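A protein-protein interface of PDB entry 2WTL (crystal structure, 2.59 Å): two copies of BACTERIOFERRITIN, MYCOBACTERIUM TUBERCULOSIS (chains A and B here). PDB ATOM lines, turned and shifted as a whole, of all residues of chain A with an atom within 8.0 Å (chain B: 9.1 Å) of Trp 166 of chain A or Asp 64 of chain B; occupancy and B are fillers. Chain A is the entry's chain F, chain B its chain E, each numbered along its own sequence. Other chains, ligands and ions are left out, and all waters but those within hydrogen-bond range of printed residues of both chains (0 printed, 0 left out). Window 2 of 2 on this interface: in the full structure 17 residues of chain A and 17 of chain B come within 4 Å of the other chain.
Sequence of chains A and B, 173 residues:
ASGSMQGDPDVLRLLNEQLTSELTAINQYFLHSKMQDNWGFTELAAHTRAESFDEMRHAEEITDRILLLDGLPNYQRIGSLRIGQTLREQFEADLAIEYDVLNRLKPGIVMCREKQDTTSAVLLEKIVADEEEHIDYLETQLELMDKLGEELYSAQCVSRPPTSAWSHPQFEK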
ATOM      1  N   PHE A  30      -3.565 -37.334  -4.181  1.00  0.00           N
ATOM      2  CA  PHE A  30      -3.974 -36.014  -4.652  1.00  0.00           C
ATOM      3  C   PHE A  30      -2.792 -35.081  -4.888  1.00  0.00           C
ATOM      4  O   PHE A  30      -2.711 -34.430  -5.928  1.00  0.00           O
ATOM      5  CB  PHE A  30      -4.980 -35.345  -3.708  1.00  0.00           C
ATOM      6  CG  PHE A  30      -5.555 -34.067  -4.262  1.00  0.00           C
ATOM      7  CD1 PHE A  30      -6.587 -34.105  -5.192  1.00  0.00           C
ATOM      8  CD2 PHE A  30      -5.052 -32.834  -3.878  1.00  0.00           C
ATOM      9  CE1 PHE A  30      -7.113 -32.941  -5.718  1.00  0.00           C
ATOM     10  CE2 PHE A  30      -5.579 -31.662  -4.401  1.00  0.00           C
ATOM     11  CZ  PHE A  30      -6.608 -31.718  -5.326  1.00  0.00           C
ATOM     12  N   LYS A  34      -1.308 -33.256  -8.375  1.00  0.00           N
ATOM     13  CA  LYS A  34      -1.044 -31.831  -8.549  1.00  0.00           C
ATOM     14  C   LYS A  34       0.408 -31.614  -8.971  1.00  0.00           C
ATOM     15  O   LYS A  34       0.703 -30.755  -9.801  1.00  0.00           O
ATOM     16  CB  LYS A  34      -1.343 -31.048  -7.266  1.00  0.00           C
ATOM     17  CG  LYS A  34      -2.760 -31.201  -6.750  1.00  0.00           C
ATOM     18  CD  LYS A  34      -3.800 -30.759  -7.773  1.00  0.00           C
ATOM     19  CE  LYS A  34      -3.874 -29.249  -7.892  1.00  0.00           C
ATOM     20  NZ  LYS A  34      -5.104 -28.801  -8.602  1.00  0.00           N
ATOM     21  N   MET A  35       1.313 -32.399  -8.400  1.00  0.00           N
ATOM     22  CA  MET A  35       2.723 -32.315  -8.762  1.00  0.00           C
ATOM     23  C   MET A  35       2.979 -32.764 -10.200  1.00  0.00           C
ATOM     24  O   MET A  35       3.700 -32.100 -10.944  1.00  0.00           O
ATOM     25  CB  MET A  35       3.577 -33.119  -7.788  1.00  0.00           C
ATOM     26  CG  MET A  35       3.591 -32.538  -6.395  1.00  0.00           C
ATOM     27  SD  MET A  35       4.651 -33.577  -5.135  1.00  0.00           S
ATOM     28  CE  MET A  35       6.417 -33.376  -5.938  1.00  0.00           C
ATOM     29  N   ASP A  37       0.748 -32.735 -12.525  1.00  0.00           N
ATOM     30  CA  ASP A  37       0.137 -31.679 -13.309  1.00  0.00           C
ATOM     31  C   ASP A  37       1.112 -30.510 -13.431  1.00  0.00           C
ATOM     32  O   ASP A  37       1.306 -29.951 -14.507  1.00  0.00           O
ATOM     33  CB  ASP A  37      -1.158 -31.219 -12.647  1.00  0.00           C
ATOM     34  CG  ASP A  37      -2.192 -30.762 -13.649  1.00  0.00           C
ATOM     35  OD1 ASP A  37      -2.076 -31.131 -14.835  1.00  0.00           O
ATOM     36  OD2 ASP A  37      -3.130 -30.043 -13.248  1.00  0.00           O
ATOM     37  N   ASN A  38       1.742 -30.165 -12.315  1.00  0.00           N
ATOM     38  CA  ASN A  38       2.608 -28.999 -12.242  1.00  0.00           C
ATOM     39  C   ASN A  38       3.928 -29.201 -12.983  1.00  0.00           C
ATOM     40  O   ASN A  38       4.558 -28.234 -13.403  1.00  0.00           O
ATOM     41  CB  ASN A  38       2.839 -28.625 -10.773  1.00  0.00           C
ATOM     42  CG  ASN A  38       3.694 -27.380 -10.606  1.00  0.00           C
ATOM     43  OD1 ASN A  38       3.411 -26.327 -11.184  1.00  0.00           O
ATOM     44  ND2 ASN A  38       4.747 -27.493  -9.798  1.00  0.00           N
ATOM     45  N   THR A  42       0.383 -33.641 -17.586  1.00  0.00           N
ATOM     46  CA  THR A  42      -1.031 -33.367 -17.361  1.00  0.00           C
ATOM     47  C   THR A  42      -1.955 -34.539 -17.707  1.00  0.00           C
ATOM     48  O   THR A  42      -3.048 -34.664 -17.147  1.00  0.00           O
ATOM     49  CB  THR A  42      -1.461 -32.133 -18.155  1.00  0.00           C
ATOM     50  OG1 THR A  42      -1.160 -32.336 -19.541  1.00  0.00           O
ATOM     51  CG2 THR A  42      -0.709 -30.908 -17.665  1.00  0.00           C
ATOM     52  N   ARG A  49      -5.419 -38.261 -10.385  1.00  0.00           N
ATOM     53  CA  ARG A  49      -6.480 -37.518  -9.713  1.00  0.00           C
ATOM     54  C   ARG A  49      -7.710 -38.396  -9.476  1.00  0.00           C
ATOM     55  O   ARG A  49      -8.315 -38.364  -8.397  1.00  0.00           O
ATOM     56  CB  ARG A  49      -6.867 -36.282 -10.524  1.00  0.00           C
ATOM     57  CG  ARG A  49      -7.938 -35.422  -9.875  1.00  0.00           C
ATOM     58  CD  ARG A  49      -8.303 -34.251 -10.769  1.00  0.00           C
ATOM     59  NE  ARG A  49      -9.243 -33.338 -10.129  1.00  0.00           N
ATOM     60  CZ  ARG A  49      -8.880 -32.283  -9.406  1.00  0.00           C
ATOM     61  NH1 ARG A  49      -7.592 -32.021  -9.225  1.00  0.00           N
ATOM     62  NH2 ARG A  49      -9.798 -31.493  -8.859  1.00  0.00           N
ATOM     63  N   THR A 163       1.372 -28.842 -22.184  1.00  0.00           N
ATOM     64  CA  THR A 163       0.850 -27.685 -21.467  1.00  0.00           C
ATOM     65  C   THR A 163       1.331 -27.689 -20.019  1.00  0.00           C
ATOM     66  O   THR A 163       2.386 -28.243 -19.709  1.00  0.00           O
ATOM     67  CB  THR A 163      -0.685 -27.651 -21.500  1.00  0.00           C
ATOM     68  OG1 THR A 163      -1.130 -27.560 -22.863  1.00  0.00           O
ATOM     69  CG2 THR A 163      -1.204 -26.445 -20.727  1.00  0.00           C
ATOM     70  N   SER A 164       0.563 -27.059 -19.139  1.00  0.00           N
ATOM     71  CA  SER A 164       0.890 -27.039 -17.720  1.00  0.00           C
ATOM     72  C   SER A 164      -0.393 -27.096 -16.906  1.00  0.00           C
ATOM     73  O   SER A 164      -1.473 -27.315 -17.456  1.00  0.00           O
ATOM     74  CB  SER A 164       1.705 -25.794 -17.363  1.00  0.00           C
ATOM     75  OG  SER A 164       1.012 -24.604 -17.697  1.00  0.00           O
ATOM     76  N   ALA A 165      -0.274 -26.898 -15.600  1.00  0.00           N
ATOM     77  CA  ALA A 165      -1.430 -26.970 -14.714  1.00  0.00           C
ATOM     78  C   ALA A 165      -2.495 -25.937 -15.082  1.00  0.00           C
ATOM     79  O   ALA A 165      -3.647 -26.045 -14.658  1.00  0.00           O
ATOM     80  CB  ALA A 165      -0.995 -26.796 -13.266  1.00  0.00           C
ATOM     81  N   TRP A 166      -2.112 -24.946 -15.878  1.00  0.00           N
ATOM     82  CA  TRP A 166      -3.001 -23.832 -16.191  1.00  0.00           C
ATOM     83  C   TRP A 166      -3.155 -23.595 -17.695  1.00  0.00           C
ATOM     84  O   TRP A 166      -2.315 -22.953 -18.330  1.00  0.00           O
ATOM     85  CB  TRP A 166      -2.504 -22.566 -15.491  1.00  0.00           C
ATOM     86  CG  TRP A 166      -2.279 -22.779 -14.026  1.00  0.00           C
ATOM     87  CD1 TRP A 166      -1.136 -23.231 -13.428  1.00  0.00           C
ATOM     88  CD2 TRP A 166      -3.226 -22.567 -12.974  1.00  0.00           C
ATOM     89  NE1 TRP A 166      -1.313 -23.307 -12.066  1.00  0.00           N
ATOM     90  CE2 TRP A 166      -2.588 -22.906 -11.763  1.00  0.00           C
ATOM     91  CE3 TRP A 166      -4.551 -22.121 -12.937  1.00  0.00           C
ATOM     92  CZ2 TRP A 166      -3.227 -22.808 -10.531  1.00  0.00           C
ATOM     93  CZ3 TRP A 166      -5.185 -22.026 -11.712  1.00  0.00           C
ATOM     94  CH2 TRP A 166      -4.524 -22.368 -10.525  1.00  0.00           C
ATOM     95  N   LEU B  12       4.392 -18.002   1.832  1.00  0.00           N
ATOM     96  CA  LEU B  12       4.268 -19.451   1.697  1.00  0.00           C
ATOM     97  C   LEU B  12       3.841 -20.103   3.011  1.00  0.00           C
ATOM     98  O   LEU B  12       3.055 -21.053   3.030  1.00  0.00           O
ATOM     99  CB  LEU B  12       5.581 -20.062   1.210  1.00  0.00           C
ATOM    100  CG  LEU B  12       5.805 -20.007  -0.300  1.00  0.00           C
ATOM    101  CD1 LEU B  12       7.157 -20.586  -0.689  1.00  0.00           C
ATOM    102  CD2 LEU B  12       4.678 -20.738  -1.012  1.00  0.00           C
ATOM    103  N   LEU B  15       0.168 -19.331   3.599  1.00  0.00           N
ATOM    104  CA  LEU B  15      -0.620 -20.164   2.703  1.00  0.00           C
ATOM    105  C   LEU B  15      -0.716 -21.588   3.231  1.00  0.00           C
ATOM    106  O   LEU B  15      -1.797 -22.170   3.270  1.00  0.00           O
ATOM    107  CB  LEU B  15      -0.030 -20.141   1.290  1.00  0.00           C
ATOM    108  CG  LEU B  15      -0.273 -18.848   0.498  1.00  0.00           C
ATOM    109  CD1 LEU B  15       0.344 -18.922  -0.883  1.00  0.00           C
ATOM    110  CD2 LEU B  15      -1.760 -18.534   0.405  1.00  0.00           C
ATOM    111  N   LEU B  19      -3.896 -23.760   4.449  1.00  0.00           N
ATOM    112  CA  LEU B  19      -4.137 -25.088   3.889  1.00  0.00           C
ATOM    113  C   LEU B  19      -4.390 -26.113   4.994  1.00  0.00           C
ATOM    114  O   LEU B  19      -5.279 -26.951   4.877  1.00  0.00           O
ATOM    115  CB  LEU B  19      -2.971 -25.545   3.001  1.00  0.00           C
ATOM    116  CG  LEU B  19      -3.093 -26.960   2.418  1.00  0.00           C
ATOM    117  CD1 LEU B  19      -4.357 -27.108   1.584  1.00  0.00           C
ATOM    118  CD2 LEU B  19      -1.860 -27.334   1.603  1.00  0.00           C
ATOM    119  N   MET B  56     -13.033 -28.005   0.081  1.00  0.00           N
ATOM    120  CA  MET B  56     -12.169 -28.775  -0.804  1.00  0.00           C
ATOM    121  C   MET B  56     -11.688 -27.898  -1.939  1.00  0.00           C
ATOM    122  O   MET B  56     -10.534 -27.976  -2.352  1.00  0.00           O
ATOM    123  CB  MET B  56     -12.923 -29.958  -1.399  1.00  0.00           C
ATOM    124  CG  MET B  56     -13.561 -30.848  -0.375  1.00  0.00           C
ATOM    125  SD  MET B  56     -13.881 -32.650  -1.051  1.00  0.00           S
ATOM    126  CE  MET B  56     -14.826 -33.259   0.522  1.00  0.00           C
ATOM    127  N   ARG B  57     -12.602 -27.082  -2.452  1.00  0.00           N
ATOM    128  CA  ARG B  57     -12.304 -26.156  -3.530  1.00  0.00           C
ATOM    129  C   ARG B  57     -11.279 -25.125  -3.069  1.00  0.00           C
ATOM    130  O   ARG B  57     -10.369 -24.770  -3.820  1.00  0.00           O
ATOM    131  CB  ARG B  57     -13.588 -25.467  -3.998  1.00  0.00           C
ATOM    132  CG  ARG B  57     -13.418 -24.558  -5.199  1.00  0.00           C
ATOM    133  CD  ARG B  57     -14.736 -23.875  -5.548  1.00  0.00           C
ATOM    134  NE  ARG B  57     -15.249 -23.070  -4.440  1.00  0.00           N
ATOM    135  CZ  ARG B  57     -14.816 -21.845  -4.149  1.00  0.00           C
ATOM    136  NH1 ARG B  57     -13.856 -21.288  -4.883  1.00  0.00           N
ATOM    137  NH2 ARG B  57     -15.334 -21.179  -3.121  1.00  0.00           N
ATOM    138  N   HIS B  58     -11.428 -24.647  -1.834  1.00  0.00           N
ATOM    139  CA  HIS B  58     -10.457 -23.726  -1.252  1.00  0.00           C
ATOM    140  C   HIS B  58      -9.089 -24.387  -1.144  1.00  0.00           C
ATOM    141  O   HIS B  58      -8.085 -23.829  -1.587  1.00  0.00           O
ATOM    142  CB  HIS B  58     -10.903 -23.248   0.133  1.00  0.00           C
ATOM    143  CG  HIS B  58     -12.013 -22.245   0.101  1.00  0.00           C
ATOM    144  ND1 HIS B  58     -12.826 -21.997   1.188  1.00  0.00           N
ATOM    145  CD2 HIS B  58     -12.450 -21.431  -0.888  1.00  0.00           C
ATOM    146  CE1 HIS B  58     -13.711 -21.070   0.870  1.00  0.00           C
ATOM    147  NE2 HIS B  58     -13.507 -20.712  -0.384  1.00  0.00           N
ATOM    148  N   ALA B  59      -9.057 -25.570  -0.543  1.00  0.00           N
ATOM    149  CA  ALA B  59      -7.818 -26.323  -0.397  1.00  0.00           C
ATOM    150  C   ALA B  59      -7.074 -26.443  -1.727  1.00  0.00           C
ATOM    151  O   ALA B  59      -5.860 -26.241  -1.789  1.00  0.00           O
ATOM    152  CB  ALA B  59      -8.100 -27.699   0.187  1.00  0.00           C
ATOM    153  N   GLU B  60      -7.802 -26.763  -2.794  1.00  0.00           N
ATOM    154  CA  GLU B  60      -7.174 -26.915  -4.098  1.00  0.00           C
ATOM    155  C   GLU B  60      -6.625 -25.583  -4.617  1.00  0.00           C
ATOM    156  O   GLU B  60      -5.517 -25.526  -5.150  1.00  0.00           O
ATOM    157  CB  GLU B  60      -8.139 -27.543  -5.105  1.00  0.00           C
ATOM    158  CG  GLU B  60      -7.480 -27.911  -6.417  1.00  0.00           C
ATOM    159  CD  GLU B  60      -8.351 -28.786  -7.293  1.00  0.00           C
ATOM    160  OE1 GLU B  60      -9.568 -28.894  -7.025  1.00  0.00           O
ATOM    161  OE2 GLU B  60      -7.816 -29.370  -8.257  1.00  0.00           O
ATOM    162  N   GLU B  61      -7.396 -24.513  -4.449  1.00  0.00           N
ATOM    163  CA  GLU B  61      -6.955 -23.189  -4.872  1.00  0.00           C
ATOM    164  C   GLU B  61      -5.648 -22.772  -4.194  1.00  0.00           C
ATOM    165  O   GLU B  61      -4.772 -22.186  -4.826  1.00  0.00           O
ATOM    166  CB  GLU B  61      -8.049 -22.150  -4.624  1.00  0.00           C
ATOM    167  CG  GLU B  61      -9.182 -22.199  -5.635  1.00  0.00           C
ATOM    168  CD  GLU B  61     -10.370 -21.337  -5.229  1.00  0.00           C
ATOM    169  OE1 GLU B  61     -10.552 -21.105  -4.010  1.00  0.00           O
ATOM    170  OE2 GLU B  61     -11.124 -20.899  -6.129  1.00  0.00           O
ATOM    171  N   ILE B  62      -5.525 -23.085  -2.908  1.00  0.00           N
ATOM    172  CA  ILE B  62      -4.326 -22.759  -2.142  1.00  0.00           C
ATOM    173  C   ILE B  62      -3.149 -23.641  -2.555  1.00  0.00           C
ATOM    174  O   ILE B  62      -2.025 -23.166  -2.715  1.00  0.00           O
ATOM    175  CB  ILE B  62      -4.574 -22.900  -0.624  1.00  0.00           C
ATOM    176  CG1 ILE B  62      -5.615 -21.876  -0.159  1.00  0.00           C
ATOM    177  CG2 ILE B  62      -3.281 -22.730   0.148  1.00  0.00           C
ATOM    178  CD1 ILE B  62      -6.109 -22.109   1.259  1.00  0.00           C
ATOM    179  N   THR B  63      -3.416 -24.932  -2.720  1.00  0.00           N
ATOM    180  CA  THR B  63      -2.414 -25.864  -3.204  1.00  0.00           C
ATOM    181  C   THR B  63      -1.812 -25.367  -4.517  1.00  0.00           C
ATOM    182  O   THR B  63      -0.592 -25.353  -4.687  1.00  0.00           O
ATOM    183  CB  THR B  63      -3.028 -27.246  -3.422  1.00  0.00           C
ATOM    184  OG1 THR B  63      -3.595 -27.711  -2.190  1.00  0.00           O
ATOM    185  CG2 THR B  63      -1.980 -28.234  -3.905  1.00  0.00           C
ATOM    186  N   ASP B  64      -2.680 -24.958  -5.438  1.00  0.00           N
ATOM    187  CA  ASP B  64      -2.260 -24.409  -6.722  1.00  0.00           C
ATOM    188  C   ASP B  64      -1.368 -23.184  -6.551  1.00  0.00           C
ATOM    189  O   ASP B  64      -0.304 -23.091  -7.162  1.00  0.00           O
ATOM    190  CB  ASP B  64      -3.481 -24.018  -7.553  1.00  0.00           C
ATOM    191  CG  ASP B  64      -4.209 -25.214  -8.127  1.00  0.00           C
ATOM    192  OD1 ASP B  64      -3.685 -26.344  -8.039  1.00  0.00           O
ATOM    193  OD2 ASP B  64      -5.315 -25.020  -8.675  1.00  0.00           O
ATOM    194  N   ARG B  65      -1.812 -22.232  -5.734  1.00  0.00           N
ATOM    195  CA  ARG B  65      -1.033 -21.023  -5.501  1.00  0.00           C
ATOM    196  C   ARG B  65       0.350 -21.372  -4.964  1.00  0.00           C
ATOM    197  O   ARG B  65       1.357 -20.820  -5.414  1.00  0.00           O
ATOM    198  CB  ARG B  65      -1.758 -20.082  -4.542  1.00  0.00           C
ATOM    199  CG  ARG B  65      -1.115 -18.712  -4.418  1.00  0.00           C
ATOM    200  CD  ARG B  65      -0.874 -18.093  -5.787  1.00  0.00           C
ATOM    201  NE  ARG B  65      -0.178 -16.811  -5.708  1.00  0.00           N
ATOM    202  CZ  ARG B  65       0.454 -16.241  -6.731  1.00  0.00           C
ATOM    203  NH1 ARG B  65       0.485 -16.843  -7.911  1.00  0.00           N
ATOM    204  NH2 ARG B  65       1.063 -15.071  -6.576  1.00  0.00           N
ATOM    205  N   ILE B  66       0.393 -22.301  -4.011  1.00  0.00           N
ATOM    206  CA  ILE B  66       1.651 -22.733  -3.407  1.00  0.00           C
ATOM    207  C   ILE B  66       2.598 -23.336  -4.444  1.00  0.00           C
ATOM    208  O   ILE B  66       3.776 -22.983  -4.497  1.00  0.00           O
ATOM    209  CB  ILE B  66       1.412 -23.749  -2.269  1.00  0.00           C
ATOM    210  CG1 ILE B  66       0.731 -23.064  -1.084  1.00  0.00           C
ATOM    211  CG2 ILE B  66       2.721 -24.392  -1.826  1.00  0.00           C
ATOM    212  CD1 ILE B  66       0.397 -24.000   0.050  1.00  0.00           C
ATOM    213  N   LEU B  67       2.076 -24.243  -5.268  1.00  0.00           N
ATOM    214  CA  LEU B  67       2.880 -24.896  -6.297  1.00  0.00           C
ATOM    215  C   LEU B  67       3.404 -23.891  -7.317  1.00  0.00           C
ATOM    216  O   LEU B  67       4.543 -23.988  -7.771  1.00  0.00           O
ATOM    217  CB  LEU B  67       2.075 -25.984  -7.004  1.00  0.00           C
ATOM    218  CG  LEU B  67       1.808 -27.247  -6.187  1.00  0.00           C
ATOM    219  CD1 LEU B  67       0.746 -28.112  -6.849  1.00  0.00           C
ATOM    220  CD2 LEU B  67       3.093 -28.026  -5.978  1.00  0.00           C
ATOM    221  N   LEU B  68       2.567 -22.924  -7.674  1.00  0.00           N
ATOM    222  CA  LEU B  68       2.978 -21.889  -8.608  1.00  0.00           C
ATOM    223  C   LEU B  68       4.139 -21.099  -8.013  1.00  0.00           C
ATOM    224  O   LEU B  68       5.038 -20.661  -8.732  1.00  0.00           O
ATOM    225  CB  LEU B  68       1.802 -20.968  -8.948  1.00  0.00           C
ATOM    226  CG  LEU B  68       1.972 -20.064 -10.173  1.00  0.00           C
ATOM    227  CD1 LEU B  68       0.632 -19.609 -10.698  1.00  0.00           C
ATOM    228  CD2 LEU B  68       2.845 -18.863  -9.849  1.00  0.00           C
ATOM    229  N   LEU B  69       4.126 -20.947  -6.691  1.00  0.00           N
ATOM    230  CA  LEU B  69       5.131 -20.156  -5.989  1.00  0.00           C
ATOM    231  C   LEU B  69       6.379 -20.943  -5.585  1.00  0.00           C
ATOM    232  O   LEU B  69       7.228 -20.424  -4.858  1.00  0.00           O
ATOM    233  CB  LEU B  69       4.515 -19.508  -4.749  1.00  0.00           C
ATOM    234  CG  LEU B  69       3.535 -18.361  -4.974  1.00  0.00           C
ATOM    235  CD1 LEU B  69       3.101 -17.806  -3.634  1.00  0.00           C
ATOM    236  CD2 LEU B  69       4.166 -17.277  -5.826  1.00  0.00           C
ATOM    237  N   ASP B  70       6.484 -22.187  -6.046  1.00  0.00           N
ATOM    238  CA  ASP B  70       7.661 -23.019  -5.784  1.00  0.00           C
ATOM    239  C   ASP B  70       7.717 -23.590  -4.374  1.00  0.00           C
ATOM    240  O   ASP B  70       8.773 -24.041  -3.930  1.00  0.00           O
ATOM    241  CB  ASP B  70       8.950 -22.238  -6.041  1.00  0.00           C
ATOM    242  CG  ASP B  70       9.615 -22.616  -7.348  1.00  0.00           C
ATOM    243  OD1 ASP B  70       9.036 -22.328  -8.423  1.00  0.00           O
ATOM    244  OD2 ASP B  70      10.728 -23.189  -7.294  1.00  0.00           O
ATOM    245  N   GLY B  71       6.595 -23.558  -3.666  1.00  0.00           N
ATOM    246  CA  GLY B  71       6.540 -24.127  -2.335  1.00  0.00           C
ATOM    247  C   GLY B  71       6.117 -25.579  -2.380  1.00  0.00           C
ATOM    248  O   GLY B  71       5.801 -26.105  -3.445  1.00  0.00           O
ATOM    249  N   PRO B  73       3.182 -27.874  -0.785  1.00  0.00           N
ATOM    250  CA  PRO B  73       1.943 -27.892  -0.008  1.00  0.00           C
ATOM    251  C   PRO B  73       2.014 -28.929   1.108  1.00  0.00           C
ATOM    252  O   PRO B  73       2.530 -30.022   0.896  1.00  0.00           O
ATOM    253  CB  PRO B  73       0.890 -28.302  -1.042  1.00  0.00           C
ATOM    254  CG  PRO B  73       1.487 -27.950  -2.364  1.00  0.00           C
ATOM    255  CD  PRO B  73       2.951 -28.189  -2.205  1.00  0.00           C
ATOM    256  N   TYR B  75       0.299 -31.585   3.181  1.00  0.00           N
ATOM    257  CA  TYR B  75      -0.849 -32.478   3.304  1.00  0.00           C
ATOM    258  C   TYR B  75      -0.670 -33.478   4.440  1.00  0.00           C
ATOM    259  O   TYR B  75      -1.422 -34.447   4.547  1.00  0.00           O
ATOM    260  CB  TYR B  75      -1.094 -33.222   1.989  1.00  0.00           C
ATOM    261  CG  TYR B  75      -1.923 -32.444   0.994  1.00  0.00           C
ATOM    262  CD1 TYR B  75      -1.399 -31.343   0.331  1.00  0.00           C
ATOM    263  CD2 TYR B  75      -3.234 -32.810   0.720  1.00  0.00           C
ATOM    264  CE1 TYR B  75      -2.158 -30.630  -0.579  1.00  0.00           C
ATOM    265  CE2 TYR B  75      -4.000 -32.103  -0.188  1.00  0.00           C
ATOM    266  CZ  TYR B  75      -3.459 -31.015  -0.835  1.00  0.00           C
ATOM    267  OH  TYR B  75      -4.220 -30.312  -1.741  1.00  0.00           O
ATOM    268  N   THR B 119      -1.709 -11.414  -6.035  1.00  0.00           N
ATOM    269  CA  THR B 119      -2.447 -12.598  -6.464  1.00  0.00           C
ATOM    270  C   THR B 119      -2.785 -13.500  -5.276  1.00  0.00           C
ATOM    271  O   THR B 119      -3.905 -13.993  -5.163  1.00  0.00           O
ATOM    272  CB  THR B 119      -1.685 -13.387  -7.538  1.00  0.00           C
ATOM    273  OG1 THR B 119      -1.359 -12.510  -8.620  1.00  0.00           O
ATOM    274  CG2 THR B 119      -2.529 -14.538  -8.058  1.00  0.00           C
ATOM    275  N   SER B 120      -1.816 -13.707  -4.389  1.00  0.00           N
ATOM    276  CA  SER B 120      -2.068 -14.448  -3.164  1.00  0.00           C
ATOM    277  C   SER B 120      -3.064 -13.691  -2.304  1.00  0.00           C
ATOM    278  O   SER B 120      -3.932 -14.286  -1.671  1.00  0.00           O
ATOM    279  CB  SER B 120      -0.770 -14.671  -2.389  1.00  0.00           C
ATOM    280  OG  SER B 120       0.061 -15.602  -3.049  1.00  0.00           O
ATOM    281  N   LEU B 123      -6.609 -14.064  -3.555  1.00  0.00           N
ATOM    282  CA  LEU B 123      -7.067 -15.409  -3.252  1.00  0.00           C
ATOM    283  C   LEU B 123      -7.637 -15.443  -1.840  1.00  0.00           C
ATOM    284  O   LEU B 123      -8.751 -15.917  -1.619  1.00  0.00           O
ATOM    285  CB  LEU B 123      -5.925 -16.413  -3.385  1.00  0.00           C
ATOM    286  CG  LEU B 123      -6.258 -17.818  -2.882  1.00  0.00           C
ATOM    287  CD1 LEU B 123      -7.340 -18.434  -3.744  1.00  0.00           C
ATOM    288  CD2 LEU B 123      -5.019 -18.714  -2.849  1.00  0.00           C
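Trp 166 of chain A touches just one residue of chain B: Asp 64 (3.2 Å).
Asp 64 of chain B touches two residues of chain A.
No residue of chain B comes within 4 Å of Ala 165 of chain A.
Of the printed residues of chain B, Lys 34 of chain A touches Glu 60, Asp 64 and Leu 67.
Of the printed residues of chain A, Leu 67 of chain B touches Lys 34.
Of the printed residues of chain A, Glu 60 of chain B touches Phe 30 (3.9 Å), Lys 34 (2.8 Å) and Arg 49 (2.8 Å).
Of the printed residues of chain A, Tyr 75 of chain B touches Phe 30 (3.3 Å).
Of the printed residues of chain B, Arg 49 of chain A touches Glu 60 (2.8 Å).
Glu 61 of chain B touches none of the printed residues of chain A.
No position is printed for both chains.
Of the 7 pairs that touch across the chains among the printed residues, none has its exchanged pair printed and touching as well.
Of the 11 printed residues of chain A, 4 touch a printed residue of chain B.
Printed residues of chain A that touch a printed residue of chain B: Phe 30, Lys 34, Arg 49 and Trp 166.
Hydrophobic or aromatic side chains of chain A that line the printed part of chain B: Phe 30 and Trp 166.
Hydrophobic or aromatic side chains of chain B within 4 Å of the printed part of chain A: Leu 67 and Tyr 75.
The side-chain hydroxyl (OG1) of Thr 63 of chain B lies within hydrogen-bond range of the side-chain hydroxyl (OH) of Tyr 75 of chain B (2.7 Å).
Among the printed residues, pairs that only touch across the chains: Trp 166 of chain A with Asp 64 of chain B (3.2 Å), Phe 30 of chain A with Tyr 75 of chain B (3.3 Å), Lys 34 of chain A with Leu 67 of chain B (3.6 Å) and Phe 30 of chain A with Glu 60 of chain B (3.9 Å).
The side-chain amino group (NZ) of Lys 34 of chain A is in salt-bridge range of the side-chain carboxylate (OE2) of Glu 60 of chain B (2.8 Å).
OE2 of Glu 60 of chain B is in salt-bridge range of NH1 of Arg 49 of chain A (2.8 Å).
OD1 of Asp 64 of chain B is in salt-bridge range of NZ of Lys 34 of chain A.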
